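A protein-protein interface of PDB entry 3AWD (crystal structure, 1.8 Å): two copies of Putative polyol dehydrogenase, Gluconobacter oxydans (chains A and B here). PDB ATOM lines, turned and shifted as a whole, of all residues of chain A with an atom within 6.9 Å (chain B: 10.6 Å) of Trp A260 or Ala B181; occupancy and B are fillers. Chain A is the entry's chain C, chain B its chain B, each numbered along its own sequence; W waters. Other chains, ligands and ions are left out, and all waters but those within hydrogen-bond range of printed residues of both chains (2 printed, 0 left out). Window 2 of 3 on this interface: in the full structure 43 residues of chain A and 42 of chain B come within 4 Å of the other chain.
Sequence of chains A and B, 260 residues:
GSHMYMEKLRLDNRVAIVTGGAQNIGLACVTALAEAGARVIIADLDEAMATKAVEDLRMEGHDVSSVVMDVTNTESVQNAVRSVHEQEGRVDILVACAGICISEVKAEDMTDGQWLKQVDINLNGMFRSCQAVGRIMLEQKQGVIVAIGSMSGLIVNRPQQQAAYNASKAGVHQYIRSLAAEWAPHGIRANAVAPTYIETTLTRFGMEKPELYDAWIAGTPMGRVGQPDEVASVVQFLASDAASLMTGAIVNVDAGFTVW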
ATOM      1  N   ILE A 155      -0.342 -20.112 -23.620  1.00  0.00           N
ATOM      2  CA  ILE A 155      -0.929 -21.242 -24.351  1.00  0.00           C
ATOM      3  C   ILE A 155      -0.713 -21.070 -25.856  1.00  0.00           C
ATOM      4  O   ILE A 155      -0.298 -20.007 -26.308  1.00  0.00           O
ATOM      5  CB  ILE A 155      -2.426 -21.477 -24.006  1.00  0.00           C
ATOM      6  CG1 ILE A 155      -3.296 -20.228 -24.277  1.00  0.00           C
ATOM      7  CG2 ILE A 155      -2.559 -21.975 -22.554  1.00  0.00           C
ATOM      8  CD1 ILE A 155      -3.547 -19.918 -25.730  1.00  0.00           C
ATOM      9  N   ILE A 217     -14.332 -19.134 -30.137  1.00  0.00           N
ATOM     10  CA  ILE A 217     -15.511 -19.076 -29.263  1.00  0.00           C
ATOM     11  C   ILE A 217     -15.714 -20.384 -28.462  1.00  0.00           C
ATOM     12  O   ILE A 217     -15.968 -20.347 -27.244  1.00  0.00           O
ATOM     13  CB  ILE A 217     -16.787 -18.748 -30.092  1.00  0.00           C
ATOM     14  CG1 ILE A 217     -16.672 -17.347 -30.747  1.00  0.00           C
ATOM     15  CG2 ILE A 217     -18.048 -18.918 -29.239  1.00  0.00           C
ATOM     16  CD1 ILE A 217     -16.359 -16.211 -29.810  1.00  0.00           C
ATOM     17  N   ALA A 218     -15.587 -21.527 -29.135  1.00  0.00           N
ATOM     18  CA  ALA A 218     -15.756 -22.824 -28.472  1.00  0.00           C
ATOM     19  C   ALA A 218     -14.710 -23.029 -27.376  1.00  0.00           C
ATOM     20  O   ALA A 218     -14.952 -23.745 -26.406  1.00  0.00           O
ATOM     21  CB  ALA A 218     -15.710 -23.974 -29.497  1.00  0.00           C
ATOM     22  N   GLY A 219     -13.543 -22.398 -27.533  1.00  0.00           N
ATOM     23  CA  GLY A 219     -12.460 -22.516 -26.571  1.00  0.00           C
ATOM     24  C   GLY A 219     -12.538 -21.531 -25.409  1.00  0.00           C
ATOM     25  O   GLY A 219     -11.688 -21.567 -24.515  1.00  0.00           O
ATOM     26  N   THR A 220     -13.563 -20.669 -25.423  1.00  0.00           N
ATOM     27  CA  THR A 220     -13.682 -19.552 -24.455  1.00  0.00           C
ATOM     28  C   THR A 220     -14.872 -19.752 -23.510  1.00  0.00           C
ATOM     29  O   THR A 220     -16.018 -19.860 -23.974  1.00  0.00           O
ATOM     30  CB  THR A 220     -13.867 -18.180 -25.180  1.00  0.00           C
ATOM     31  OG1 THR A 220     -12.792 -17.961 -26.107  1.00  0.00           O
ATOM     32  CG2 THR A 220     -13.861 -17.035 -24.161  1.00  0.00           C
ATOM     33  N   PRO A 221     -14.610 -19.834 -22.192  1.00  0.00           N
ATOM     34  CA  PRO A 221     -15.715 -20.008 -21.233  1.00  0.00           C
ATOM     35  C   PRO A 221     -16.812 -18.930 -21.342  1.00  0.00           C
ATOM     36  O   PRO A 221     -17.996 -19.282 -21.292  1.00  0.00           O
ATOM     37  CB  PRO A 221     -14.998 -19.997 -19.873  1.00  0.00           C
ATOM     38  CG  PRO A 221     -13.628 -20.609 -20.210  1.00  0.00           C
ATOM     39  CD  PRO A 221     -13.294 -19.900 -21.518  1.00  0.00           C
ATOM     40  N   MET A 222     -16.439 -17.653 -21.491  1.00  0.00           N
ATOM     41  CA  MET A 222     -17.444 -16.578 -21.711  1.00  0.00           C
ATOM     42  C   MET A 222     -18.111 -16.626 -23.095  1.00  0.00           C
ATOM     43  O   MET A 222     -19.067 -15.870 -23.369  1.00  0.00           O
ATOM     44  CB  MET A 222     -16.830 -15.190 -21.508  1.00  0.00           C
ATOM     45  CG  MET A 222     -16.454 -14.839 -20.093  1.00  0.00           C
ATOM     46  SD  MET A 222     -15.951 -13.095 -19.999  1.00  0.00           S
ATOM     47  CE  MET A 222     -15.626 -12.997 -18.239  1.00  0.00           C
ATOM     48  N   GLY A 223     -17.601 -17.476 -23.983  1.00  0.00           N
ATOM     49  CA  GLY A 223     -18.218 -17.665 -25.315  1.00  0.00           C
ATOM     50  C   GLY A 223     -18.187 -16.424 -26.197  1.00  0.00           C
ATOM     51  O   GLY A 223     -19.073 -16.232 -27.034  1.00  0.00           O
ATOM     52  N   GLY A 256     -11.424 -16.325 -19.568  1.00  0.00           N
ATOM     53  CA  GLY A 256     -11.266 -17.683 -19.061  1.00  0.00           C
ATOM     54  C   GLY A 256     -10.599 -18.649 -20.033  1.00  0.00           C
ATOM     55  O   GLY A 256     -10.548 -19.851 -19.770  1.00  0.00           O
ATOM     56  N   PHE A 257     -10.062 -18.137 -21.143  1.00  0.00           N
ATOM     57  CA  PHE A 257      -9.546 -19.028 -22.180  1.00  0.00           C
ATOM     58  C   PHE A 257      -8.450 -19.964 -21.630  1.00  0.00           C
ATOM     59  O   PHE A 257      -8.420 -21.149 -21.975  1.00  0.00           O
ATOM     60  CB  PHE A 257      -8.999 -18.213 -23.361  1.00  0.00           C
ATOM     61  CG  PHE A 257      -8.706 -19.037 -24.574  1.00  0.00           C
ATOM     62  CD1 PHE A 257      -9.659 -19.163 -25.587  1.00  0.00           C
ATOM     63  CD2 PHE A 257      -7.469 -19.685 -24.711  1.00  0.00           C
ATOM     64  CE1 PHE A 257      -9.396 -19.931 -26.730  1.00  0.00           C
ATOM     65  CE2 PHE A 257      -7.195 -20.455 -25.849  1.00  0.00           C
ATOM     66  CZ  PHE A 257      -8.167 -20.581 -26.852  1.00  0.00           C
ATOM     67  N   THR A 258      -7.559 -19.418 -20.803  1.00  0.00           N
ATOM     68  CA  THR A 258      -6.456 -20.210 -20.217  1.00  0.00           C
ATOM     69  C   THR A 258      -6.908 -21.103 -19.060  1.00  0.00           C
ATOM     70  O   THR A 258      -6.095 -21.849 -18.500  1.00  0.00           O
ATOM     71  CB  THR A 258      -5.301 -19.320 -19.742  1.00  0.00           C
ATOM     72  OG1 THR A 258      -5.771 -18.374 -18.764  1.00  0.00           O
ATOM     73  CG2 THR A 258      -4.701 -18.551 -20.940  1.00  0.00           C
ATOM     74  N   VAL A 259      -8.168 -20.978 -18.657  1.00  0.00           N
ATOM     75  CA  VAL A 259      -8.692 -21.795 -17.534  1.00  0.00           C
ATOM     76  C   VAL A 259      -8.954 -23.242 -17.972  1.00  0.00           C
ATOM     77  O   VAL A 259      -8.723 -24.198 -17.221  1.00  0.00           O
ATOM     78  CB  VAL A 259      -9.967 -21.170 -16.932  1.00  0.00           C
ATOM     79  CG1 VAL A 259     -10.559 -22.082 -15.846  1.00  0.00           C
ATOM     80  CG2 VAL A 259      -9.662 -19.765 -16.355  1.00  0.00           C
ATOM     81  N   TRP A 260      -9.463 -23.394 -19.184  1.00  0.00           N
ATOM     82  CA  TRP A 260      -9.689 -24.724 -19.743  1.00  0.00           C
ATOM     83  C   TRP A 260      -8.394 -25.303 -20.308  1.00  0.00           C
ATOM     84  O   TRP A 260      -8.253 -26.531 -20.470  1.00  0.00           O
ATOM     85  CB  TRP A 260     -10.711 -24.625 -20.872  1.00  0.00           C
ATOM     86  CG  TRP A 260     -12.144 -24.600 -20.438  1.00  0.00           C
ATOM     87  CD1 TRP A 260     -12.677 -25.064 -19.261  1.00  0.00           C
ATOM     88  CD2 TRP A 260     -13.253 -24.134 -21.225  1.00  0.00           C
ATOM     89  NE1 TRP A 260     -14.053 -24.909 -19.277  1.00  0.00           N
ATOM     90  CE2 TRP A 260     -14.427 -24.345 -20.469  1.00  0.00           C
ATOM     91  CE3 TRP A 260     -13.366 -23.574 -22.510  1.00  0.00           C
ATOM     92  CZ2 TRP A 260     -15.713 -23.999 -20.952  1.00  0.00           C
ATOM     93  CZ3 TRP A 260     -14.628 -23.226 -22.986  1.00  0.00           C
ATOM     94  CH2 TRP A 260     -15.785 -23.443 -22.206  1.00  0.00           C
ATOM     95  OXT TRP A 260      -7.446 -24.554 -20.656  1.00  0.00           O
ATOM     96  N   LEU B 138     -26.517 -17.280  -9.656  1.00  0.00           N
ATOM     97  CA  LEU B 138     -27.068 -18.044 -10.772  1.00  0.00           C
ATOM     98  C   LEU B 138     -28.527 -17.669 -11.086  1.00  0.00           C
ATOM     99  O   LEU B 138     -28.924 -17.541 -12.263  1.00  0.00           O
ATOM    100  CB  LEU B 138     -26.933 -19.539 -10.498  1.00  0.00           C
ATOM    101  CG  LEU B 138     -25.492 -20.046 -10.624  1.00  0.00           C
ATOM    102  CD1 LEU B 138     -25.377 -21.471 -10.098  1.00  0.00           C
ATOM    103  CD2 LEU B 138     -24.985 -19.972 -12.081  1.00  0.00           C
ATOM    104  N   ILE B 145     -17.269 -12.924  -7.855  1.00  0.00           N
ATOM    105  CA  ILE B 145     -16.588 -13.419  -6.680  1.00  0.00           C
ATOM    106  C   ILE B 145     -15.137 -12.990  -6.785  1.00  0.00           C
ATOM    107  O   ILE B 145     -14.525 -13.092  -7.869  1.00  0.00           O
ATOM    108  CB  ILE B 145     -16.674 -14.965  -6.581  1.00  0.00           C
ATOM    109  CG1 ILE B 145     -18.137 -15.398  -6.345  1.00  0.00           C
ATOM    110  CG2 ILE B 145     -15.762 -15.497  -5.472  1.00  0.00           C
ATOM    111  CD1 ILE B 145     -18.402 -16.886  -6.573  1.00  0.00           C
ATOM    112  N   HIS B 173      -7.341 -21.253  -5.139  1.00  0.00           N
ATOM    113  CA  HIS B 173      -7.111 -20.744  -6.502  1.00  0.00           C
ATOM    114  C   HIS B 173      -7.799 -21.643  -7.542  1.00  0.00           C
ATOM    115  O   HIS B 173      -8.479 -21.153  -8.420  1.00  0.00           O
ATOM    116  CB  HIS B 173      -5.611 -20.662  -6.827  1.00  0.00           C
ATOM    117  CG  HIS B 173      -4.840 -19.680  -5.978  1.00  0.00           C
ATOM    118  ND1 HIS B 173      -3.470 -19.545  -6.080  1.00  0.00           N
ATOM    119  CD2 HIS B 173      -5.236 -18.801  -5.027  1.00  0.00           C
ATOM    120  CE1 HIS B 173      -3.056 -18.621  -5.225  1.00  0.00           C
ATOM    121  NE2 HIS B 173      -4.106 -18.163  -4.568  1.00  0.00           N
ATOM    122  N   GLN B 174      -7.592 -22.951  -7.461  1.00  0.00           N
ATOM    123  CA  GLN B 174      -8.131 -23.843  -8.498  1.00  0.00           C
ATOM    124  C   GLN B 174      -9.638 -24.063  -8.348  1.00  0.00           C
ATOM    125  O   GLN B 174     -10.345 -24.295  -9.335  1.00  0.00           O
ATOM    126  CB  GLN B 174      -7.344 -25.174  -8.562  1.00  0.00           C
ATOM    127  CG  GLN B 174      -7.728 -26.069  -9.786  1.00  0.00           C
ATOM    128  CD  GLN B 174      -7.327 -25.456 -11.139  1.00  0.00           C
ATOM    129  OE1 GLN B 174      -6.891 -24.310 -11.217  1.00  0.00           O
ATOM    130  NE2 GLN B 174      -7.433 -26.243 -12.194  1.00  0.00           N
ATOM    131  N   TYR B 175     -10.133 -24.003  -7.115  1.00  0.00           N
ATOM    132  CA  TYR B 175     -11.585 -24.019  -6.892  1.00  0.00           C
ATOM    133  C   TYR B 175     -12.229 -22.793  -7.581  1.00  0.00           C
ATOM    134  O   TYR B 175     -13.211 -22.933  -8.299  1.00  0.00           O
ATOM    135  CB  TYR B 175     -11.907 -24.023  -5.395  1.00  0.00           C
ATOM    136  CG  TYR B 175     -13.396 -23.930  -5.122  1.00  0.00           C
ATOM    137  CD1 TYR B 175     -14.290 -24.897  -5.635  1.00  0.00           C
ATOM    138  CD2 TYR B 175     -13.916 -22.867  -4.381  1.00  0.00           C
ATOM    139  CE1 TYR B 175     -15.685 -24.798  -5.395  1.00  0.00           C
ATOM    140  CE2 TYR B 175     -15.308 -22.756  -4.120  1.00  0.00           C
ATOM    141  CZ  TYR B 175     -16.176 -23.711  -4.647  1.00  0.00           C
ATOM    142  OH  TYR B 175     -17.527 -23.621  -4.407  1.00  0.00           O
ATOM    143  N   ILE B 176     -11.655 -21.606  -7.359  1.00  0.00           N
ATOM    144  CA  ILE B 176     -12.177 -20.365  -7.974  1.00  0.00           C
ATOM    145  C   ILE B 176     -12.146 -20.457  -9.504  1.00  0.00           C
ATOM    146  O   ILE B 176     -13.096 -20.059 -10.163  1.00  0.00           O
ATOM    147  CB  ILE B 176     -11.410 -19.140  -7.428  1.00  0.00           C
ATOM    148  CG1 ILE B 176     -11.776 -18.908  -5.947  1.00  0.00           C
ATOM    149  CG2 ILE B 176     -11.582 -17.867  -8.326  1.00  0.00           C
ATOM    150  CD1 ILE B 176     -13.228 -18.414  -5.717  1.00  0.00           C
ATOM    151  N   ARG B 177     -11.065 -21.015 -10.048  1.00  0.00           N
ATOM    152  CA  ARG B 177     -10.966 -21.230 -11.503  1.00  0.00           C
ATOM    153  C   ARG B 177     -12.048 -22.187 -12.031  1.00  0.00           C
ATOM    154  O   ARG B 177     -12.613 -21.967 -13.103  1.00  0.00           O
ATOM    155  CB  ARG B 177      -9.560 -21.717 -11.863  1.00  0.00           C
ATOM    156  CG  ARG B 177      -8.520 -20.559 -11.754  1.00  0.00           C
ATOM    157  CD  ARG B 177      -7.071 -21.089 -11.696  1.00  0.00           C
ATOM    158  NE  ARG B 177      -6.665 -21.918 -12.857  1.00  0.00           N
ATOM    159  CZ  ARG B 177      -6.297 -21.418 -14.036  1.00  0.00           C
ATOM    160  NH1 ARG B 177      -6.390 -20.114 -14.256  1.00  0.00           N
ATOM    161  NH2 ARG B 177      -5.879 -22.214 -15.015  1.00  0.00           N
ATOM    162  N   SER B 178     -12.316 -23.246 -11.262  1.00  0.00           N
ATOM    163  CA  SER B 178     -13.420 -24.171 -11.556  1.00  0.00           C
ATOM    164  C   SER B 178     -14.770 -23.452 -11.594  1.00  0.00           C
ATOM    165  O   SER B 178     -15.569 -23.697 -12.512  1.00  0.00           O
ATOM    166  CB  SER B 178     -13.460 -25.319 -10.540  1.00  0.00           C
ATOM    167  OG  SER B 178     -12.244 -26.064 -10.551  1.00  0.00           O
ATOM    168  N   LEU B 179     -15.023 -22.580 -10.611  1.00  0.00           N
ATOM    169  CA  LEU B 179     -16.253 -21.807 -10.589  1.00  0.00           C
ATOM    170  C   LEU B 179     -16.292 -20.865 -11.792  1.00  0.00           C
ATOM    171  O   LEU B 179     -17.336 -20.732 -12.439  1.00  0.00           O
ATOM    172  CB  LEU B 179     -16.404 -21.015  -9.282  1.00  0.00           C
ATOM    173  CG  LEU B 179     -16.456 -21.784  -7.963  1.00  0.00           C
ATOM    174  CD1 LEU B 179     -16.717 -20.756  -6.838  1.00  0.00           C
ATOM    175  CD2 LEU B 179     -17.546 -22.879  -8.016  1.00  0.00           C
ATOM    176  N   ALA B 180     -15.156 -20.235 -12.095  1.00  0.00           N
ATOM    177  CA  ALA B 180     -15.046 -19.323 -13.250  1.00  0.00           C
ATOM    178  C   ALA B 180     -15.500 -20.054 -14.523  1.00  0.00           C
ATOM    179  O   ALA B 180     -16.356 -19.548 -15.289  1.00  0.00           O
ATOM    180  CB  ALA B 180     -13.596 -18.798 -13.393  1.00  0.00           C
ATOM    181  N   ALA B 181     -14.996 -21.274 -14.718  1.00  0.00           N
ATOM    182  CA  ALA B 181     -15.345 -22.043 -15.920  1.00  0.00           C
ATOM    183  C   ALA B 181     -16.810 -22.466 -15.936  1.00  0.00           C
ATOM    184  O   ALA B 181     -17.494 -22.300 -16.944  1.00  0.00           O
ATOM    185  CB  ALA B 181     -14.427 -23.262 -16.080  1.00  0.00           C
ATOM    186  N   GLU B 182     -17.293 -23.011 -14.828  1.00  0.00           N
ATOM    187  CA  GLU B 182     -18.685 -23.500 -14.765  1.00  0.00           C
ATOM    188  C   GLU B 182     -19.705 -22.371 -14.920  1.00  0.00           C
ATOM    189  O   GLU B 182     -20.764 -22.586 -15.501  1.00  0.00           O
ATOM    190  CB  GLU B 182     -18.950 -24.244 -13.445  1.00  0.00           C
ATOM    191  CG  GLU B 182     -18.162 -25.555 -13.262  1.00  0.00           C
ATOM    192  CD  GLU B 182     -18.693 -26.418 -12.111  1.00  0.00           C
ATOM    193  OE1 GLU B 182     -19.928 -26.427 -11.897  1.00  0.00           O
ATOM    194  OE2 GLU B 182     -17.859 -27.074 -11.431  1.00  0.00           O
ATOM    195  N   TRP B 183     -19.398 -21.190 -14.371  1.00  0.00           N
ATOM    196  CA  TRP B 183     -20.407 -20.123 -14.234  1.00  0.00           C
ATOM    197  C   TRP B 183     -20.264 -18.980 -15.248  1.00  0.00           C
ATOM    198  O   TRP B 183     -21.125 -18.084 -15.313  1.00  0.00           O
ATOM    199  CB  TRP B 183     -20.411 -19.593 -12.784  1.00  0.00           C
ATOM    200  CG  TRP B 183     -20.890 -20.644 -11.780  1.00  0.00           C
ATOM    201  CD1 TRP B 183     -21.525 -21.828 -12.071  1.00  0.00           C
ATOM    202  CD2 TRP B 183     -20.818 -20.573 -10.352  1.00  0.00           C
ATOM    203  NE1 TRP B 183     -21.842 -22.506 -10.912  1.00  0.00           N
ATOM    204  CE2 TRP B 183     -21.423 -21.762  -9.841  1.00  0.00           C
ATOM    205  CE3 TRP B 183     -20.282 -19.639  -9.445  1.00  0.00           C
ATOM    206  CZ2 TRP B 183     -21.516 -22.024  -8.474  1.00  0.00           C
ATOM    207  CZ3 TRP B 183     -20.364 -19.904  -8.091  1.00  0.00           C
ATOM    208  CH2 TRP B 183     -20.978 -21.091  -7.614  1.00  0.00           C
ATOM    209  N   ALA B 184     -19.182 -19.006 -16.029  1.00  0.00           N
ATOM    210  CA  ALA B 184     -18.960 -18.012 -17.100  1.00  0.00           C
ATOM    211  C   ALA B 184     -20.160 -17.796 -18.049  1.00  0.00           C
ATOM    212  O   ALA B 184     -20.448 -16.661 -18.408  1.00  0.00           O
ATOM    213  CB  ALA B 184     -17.716 -18.360 -17.903  1.00  0.00           C
ATOM    214  N   PRO B 185     -20.840 -18.878 -18.484  1.00  0.00           N
ATOM    215  CA  PRO B 185     -22.004 -18.675 -19.365  1.00  0.00           C
ATOM    216  C   PRO B 185     -23.224 -18.010 -18.706  1.00  0.00           C
ATOM    217  O   PRO B 185     -24.200 -17.675 -19.397  1.00  0.00           O
ATOM    218  CB  PRO B 185     -22.376 -20.099 -19.788  1.00  0.00           C
ATOM    219  CG  PRO B 185     -21.159 -20.963 -19.470  1.00  0.00           C
ATOM    220  CD  PRO B 185     -20.566 -20.316 -18.252  1.00  0.00           C
ATOM    221  N   HIS B 186     -23.170 -17.811 -17.393  1.00  0.00           N
ATOM    222  CA  HIS B 186     -24.332 -17.362 -16.636  1.00  0.00           C
ATOM    223  C   HIS B 186     -24.102 -16.016 -15.955  1.00  0.00           C
ATOM    224  O   HIS B 186     -24.698 -15.737 -14.905  1.00  0.00           O
ATOM    225  CB  HIS B 186     -24.704 -18.434 -15.609  1.00  0.00           C
ATOM    226  CG  HIS B 186     -24.849 -19.799 -16.205  1.00  0.00           C
ATOM    227  ND1 HIS B 186     -25.771 -20.076 -17.189  1.00  0.00           N
ATOM    228  CD2 HIS B 186     -24.168 -20.950 -15.990  1.00  0.00           C
ATOM    229  CE1 HIS B 186     -25.670 -21.347 -17.541  1.00  0.00           C
ATOM    230  NE2 HIS B 186     -24.696 -21.896 -16.839  1.00  0.00           N
ATOM    231  N   GLY B 187     -23.247 -15.195 -16.566  1.00  0.00           N
ATOM    232  CA  GLY B 187     -23.028 -13.805 -16.151  1.00  0.00           C
ATOM    233  C   GLY B 187     -22.239 -13.600 -14.860  1.00  0.00           C
ATOM    234  O   GLY B 187     -22.293 -12.520 -14.268  1.00  0.00           O
ATOM    235  N   ILE B 188     -21.510 -14.629 -14.433  1.00  0.00           N
ATOM    236  CA  ILE B 188     -20.725 -14.580 -13.188  1.00  0.00           C
ATOM    237  C   ILE B 188     -19.251 -14.626 -13.541  1.00  0.00           C
ATOM    238  O   ILE B 188     -18.862 -15.383 -14.438  1.00  0.00           O
ATOM    239  CB  ILE B 188     -21.088 -15.780 -12.282  1.00  0.00           C
ATOM    240  CG1 ILE B 188     -22.570 -15.691 -11.872  1.00  0.00           C
ATOM    241  CG2 ILE B 188     -20.163 -15.881 -11.052  1.00  0.00           C
ATOM    242  CD1 ILE B 188     -23.103 -16.992 -11.293  1.00  0.00           C
ATOM    243  N   ARG B 189     -18.446 -13.809 -12.858  1.00  0.00           N
ATOM    244  CA  ARG B 189     -16.990 -13.886 -12.950  1.00  0.00           C
ATOM    245  C   ARG B 189     -16.434 -14.266 -11.593  1.00  0.00           C
ATOM    246  O   ARG B 189     -17.018 -13.919 -10.561  1.00  0.00           O
ATOM    247  CB  ARG B 189     -16.379 -12.536 -13.380  1.00  0.00           C
ATOM    248  CG  ARG B 189     -16.808 -12.068 -14.766  1.00  0.00           C
ATOM    249  CD  ARG B 189     -16.059 -10.755 -15.170  1.00  0.00           C
ATOM    250  NE  ARG B 189     -16.393  -9.622 -14.285  1.00  0.00           N
ATOM    251  CZ  ARG B 189     -15.605  -9.151 -13.303  1.00  0.00           C
ATOM    252  NH1 ARG B 189     -14.427  -9.725 -13.044  1.00  0.00           N
ATOM    253  NH2 ARG B 189     -16.020  -8.114 -12.554  1.00  0.00           N
ATOM    254  N   ALA B 190     -15.312 -14.983 -11.591  1.00  0.00           N
ATOM    255  CA  ALA B 190     -14.672 -15.362 -10.329  1.00  0.00           C
ATOM    256  C   ALA B 190     -13.161 -15.287 -10.525  1.00  0.00           C
ATOM    257  O   ALA B 190     -12.610 -15.890 -11.470  1.00  0.00           O
ATOM    258  CB  ALA B 190     -15.093 -16.764  -9.905  1.00  0.00           C
ATOM    259  N   ASN B 191     -12.511 -14.504  -9.677  1.00  0.00           N
ATOM    260  CA  ASN B 191     -11.056 -14.346  -9.724  1.00  0.00           C
ATOM    261  C   ASN B 191     -10.470 -14.384  -8.306  1.00  0.00           C
ATOM    262  O   ASN B 191     -11.203 -14.317  -7.317  1.00  0.00           O
ATOM    263  CB  ASN B 191     -10.664 -13.017 -10.392  1.00  0.00           C
ATOM    264  CG  ASN B 191     -11.136 -12.917 -11.826  1.00  0.00           C
ATOM    265  OD1 ASN B 191     -10.537 -13.504 -12.749  1.00  0.00           O
ATOM    266  ND2 ASN B 191     -12.223 -12.173 -12.033  1.00  0.00           N
ATOM    267  N   MET B 246     -12.055 -10.325 -17.280  1.00  0.00           N
ATOM    268  CA  MET B 246     -11.257 -11.188 -16.421  1.00  0.00           C
ATOM    269  C   MET B 246     -12.109 -12.220 -15.665  1.00  0.00           C
ATOM    270  O   MET B 246     -12.985 -11.854 -14.865  1.00  0.00           O
ATOM    271  CB  MET B 246     -10.448 -10.359 -15.412  1.00  0.00           C
ATOM    272  CG  MET B 246      -9.437  -9.382 -16.028  1.00  0.00           C
ATOM    273  SD  MET B 246      -8.456  -8.489 -14.806  1.00  0.00           S
ATOM    274  CE  MET B 246      -7.499  -9.819 -14.060  1.00  0.00           C
ATOM    275  N   THR B 247     -11.861 -13.504 -15.919  1.00  0.00           N
ATOM    276  CA  THR B 247     -12.415 -14.548 -15.060  1.00  0.00           C
ATOM    277  C   THR B 247     -11.424 -15.714 -14.979  1.00  0.00           C
ATOM    278  O   THR B 247     -10.725 -16.007 -15.960  1.00  0.00           O
ATOM    279  CB  THR B 247     -13.848 -14.988 -15.491  1.00  0.00           C
ATOM    280  OG1 THR B 247     -14.490 -15.663 -14.399  1.00  0.00           O
ATOM    281  CG2 THR B 247     -13.824 -15.903 -16.744  1.00  0.00           C
ATOM    282  N   GLY B 248     -11.360 -16.353 -13.814  1.00  0.00           N
ATOM    283  CA  GLY B 248     -10.401 -17.444 -13.558  1.00  0.00           C
ATOM    284  C   GLY B 248      -8.955 -16.989 -13.425  1.00  0.00           C
ATOM    285  O   GLY B 248      -8.031 -17.816 -13.471  1.00  0.00           O
ATOM    286  N   ALA B 249      -8.740 -15.678 -13.277  1.00  0.00           N
ATOM    287  CA  ALA B 249      -7.400 -15.121 -13.098  1.00  0.00           C
ATOM    288  C   ALA B 249      -6.934 -15.255 -11.649  1.00  0.00           C
ATOM    289  O   ALA B 249      -7.664 -14.907 -10.724  1.00  0.00           O
ATOM    290  CB  ALA B 249      -7.366 -13.652 -13.526  1.00  0.00           C
HETATM  291  O   HOH W   1      -5.880 -18.005 -16.080  1.00  0.00           O
HETATM  292  O   HOH W   2      -4.305 -20.834 -16.912  1.00  0.00           O
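Trp A260 touches one residue of chain B. Of chain A, only Trp A260 comes within 4 Å of Ala B181. No residue of chain B comes within 4 Å of Thr A220. Val A259 touches just these residues of chain B: Arg B177 (3.4 Å), Thr B247 (3.9 Å) and Gly B248 (3.7 Å). Of the printed residues of chain B, Thr A258 touches Arg B177 (3.5 Å). Of the printed residues of chain A, Arg B177 touches Thr A258 (3.5 Å) and Val A259 (3.4 Å). Printed residues of chain A within 4 Å of Gly B248: Val A259 (3.7 Å). The nearest residue of chain B that does not touch Trp A260 is Arg B177 (5.6 Å). The nearest residue of chain A that does not touch Ala B181 is Val A259 (4.1 Å).
O of Met B246 is in hydrogen-bond range of NH1 of Arg B189 (3.2 Å). The backbone carbonyl oxygen of Gly B248 sits at hydrogen-bond distance from the guanidinium group of Arg B177, 2.9 Å away. The side-chain hydroxyl (OG1) of Thr B247 lies within hydrogen-bond range of the backbone NH (N) of Ala B190 (3.0 Å). The backbone NH (N) of Gly B248 is in hydrogen-bond range of the side-chain amide oxygen (OD1) of Asn B191 (3.2 Å). N of Ile B145 is in hydrogen-bond range of O of Arg B189, at 2.9 Å. NE of Arg B177 sits at hydrogen-bond distance from OE1 of Gln B174, 2.9 Å away.
Water W2 lies within hydrogen-bond range of O of Thr A258 and NH2 of Arg B177. Water W1 lies within hydrogen-bond range of OG1 of Thr A258, NH1 of Arg B177 and O of Gly B248.
Printed residues of chain B that touch a printed residue of chain A: Arg B177, Ala B181, Ala B184, Arg B189, Thr B247 and Gly B248. Hydrophobic or aromatic side chains of chain A that line the printed part of chain B: Pro A221, Met A222, Val A259 and Trp A260. Among the printed residues, 10 pairs touch across the chains.
No position is printed for both chains. Of the 10 pairs that touch across the chains among the printed residues, none has its exchanged pair printed and touching as well.
Pro A221 touches Ala B184. Met A222 touches Ala B184. Arg B189 touches Met A222 (CG to CE, 3.8 Å). Met A222 touches Thr B247 (CE to CG2, 3.7 Å). Thr B247 touches Gly A256. O of Thr A258 touches NH2 of Arg B177 (3.5 Å). Val A259 touches Arg B177 (CG1 to O, 3.4 Å). Thr B247 touches Val A259. Gly B248 touches Val A259. Trp A260 touches Ala B181.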
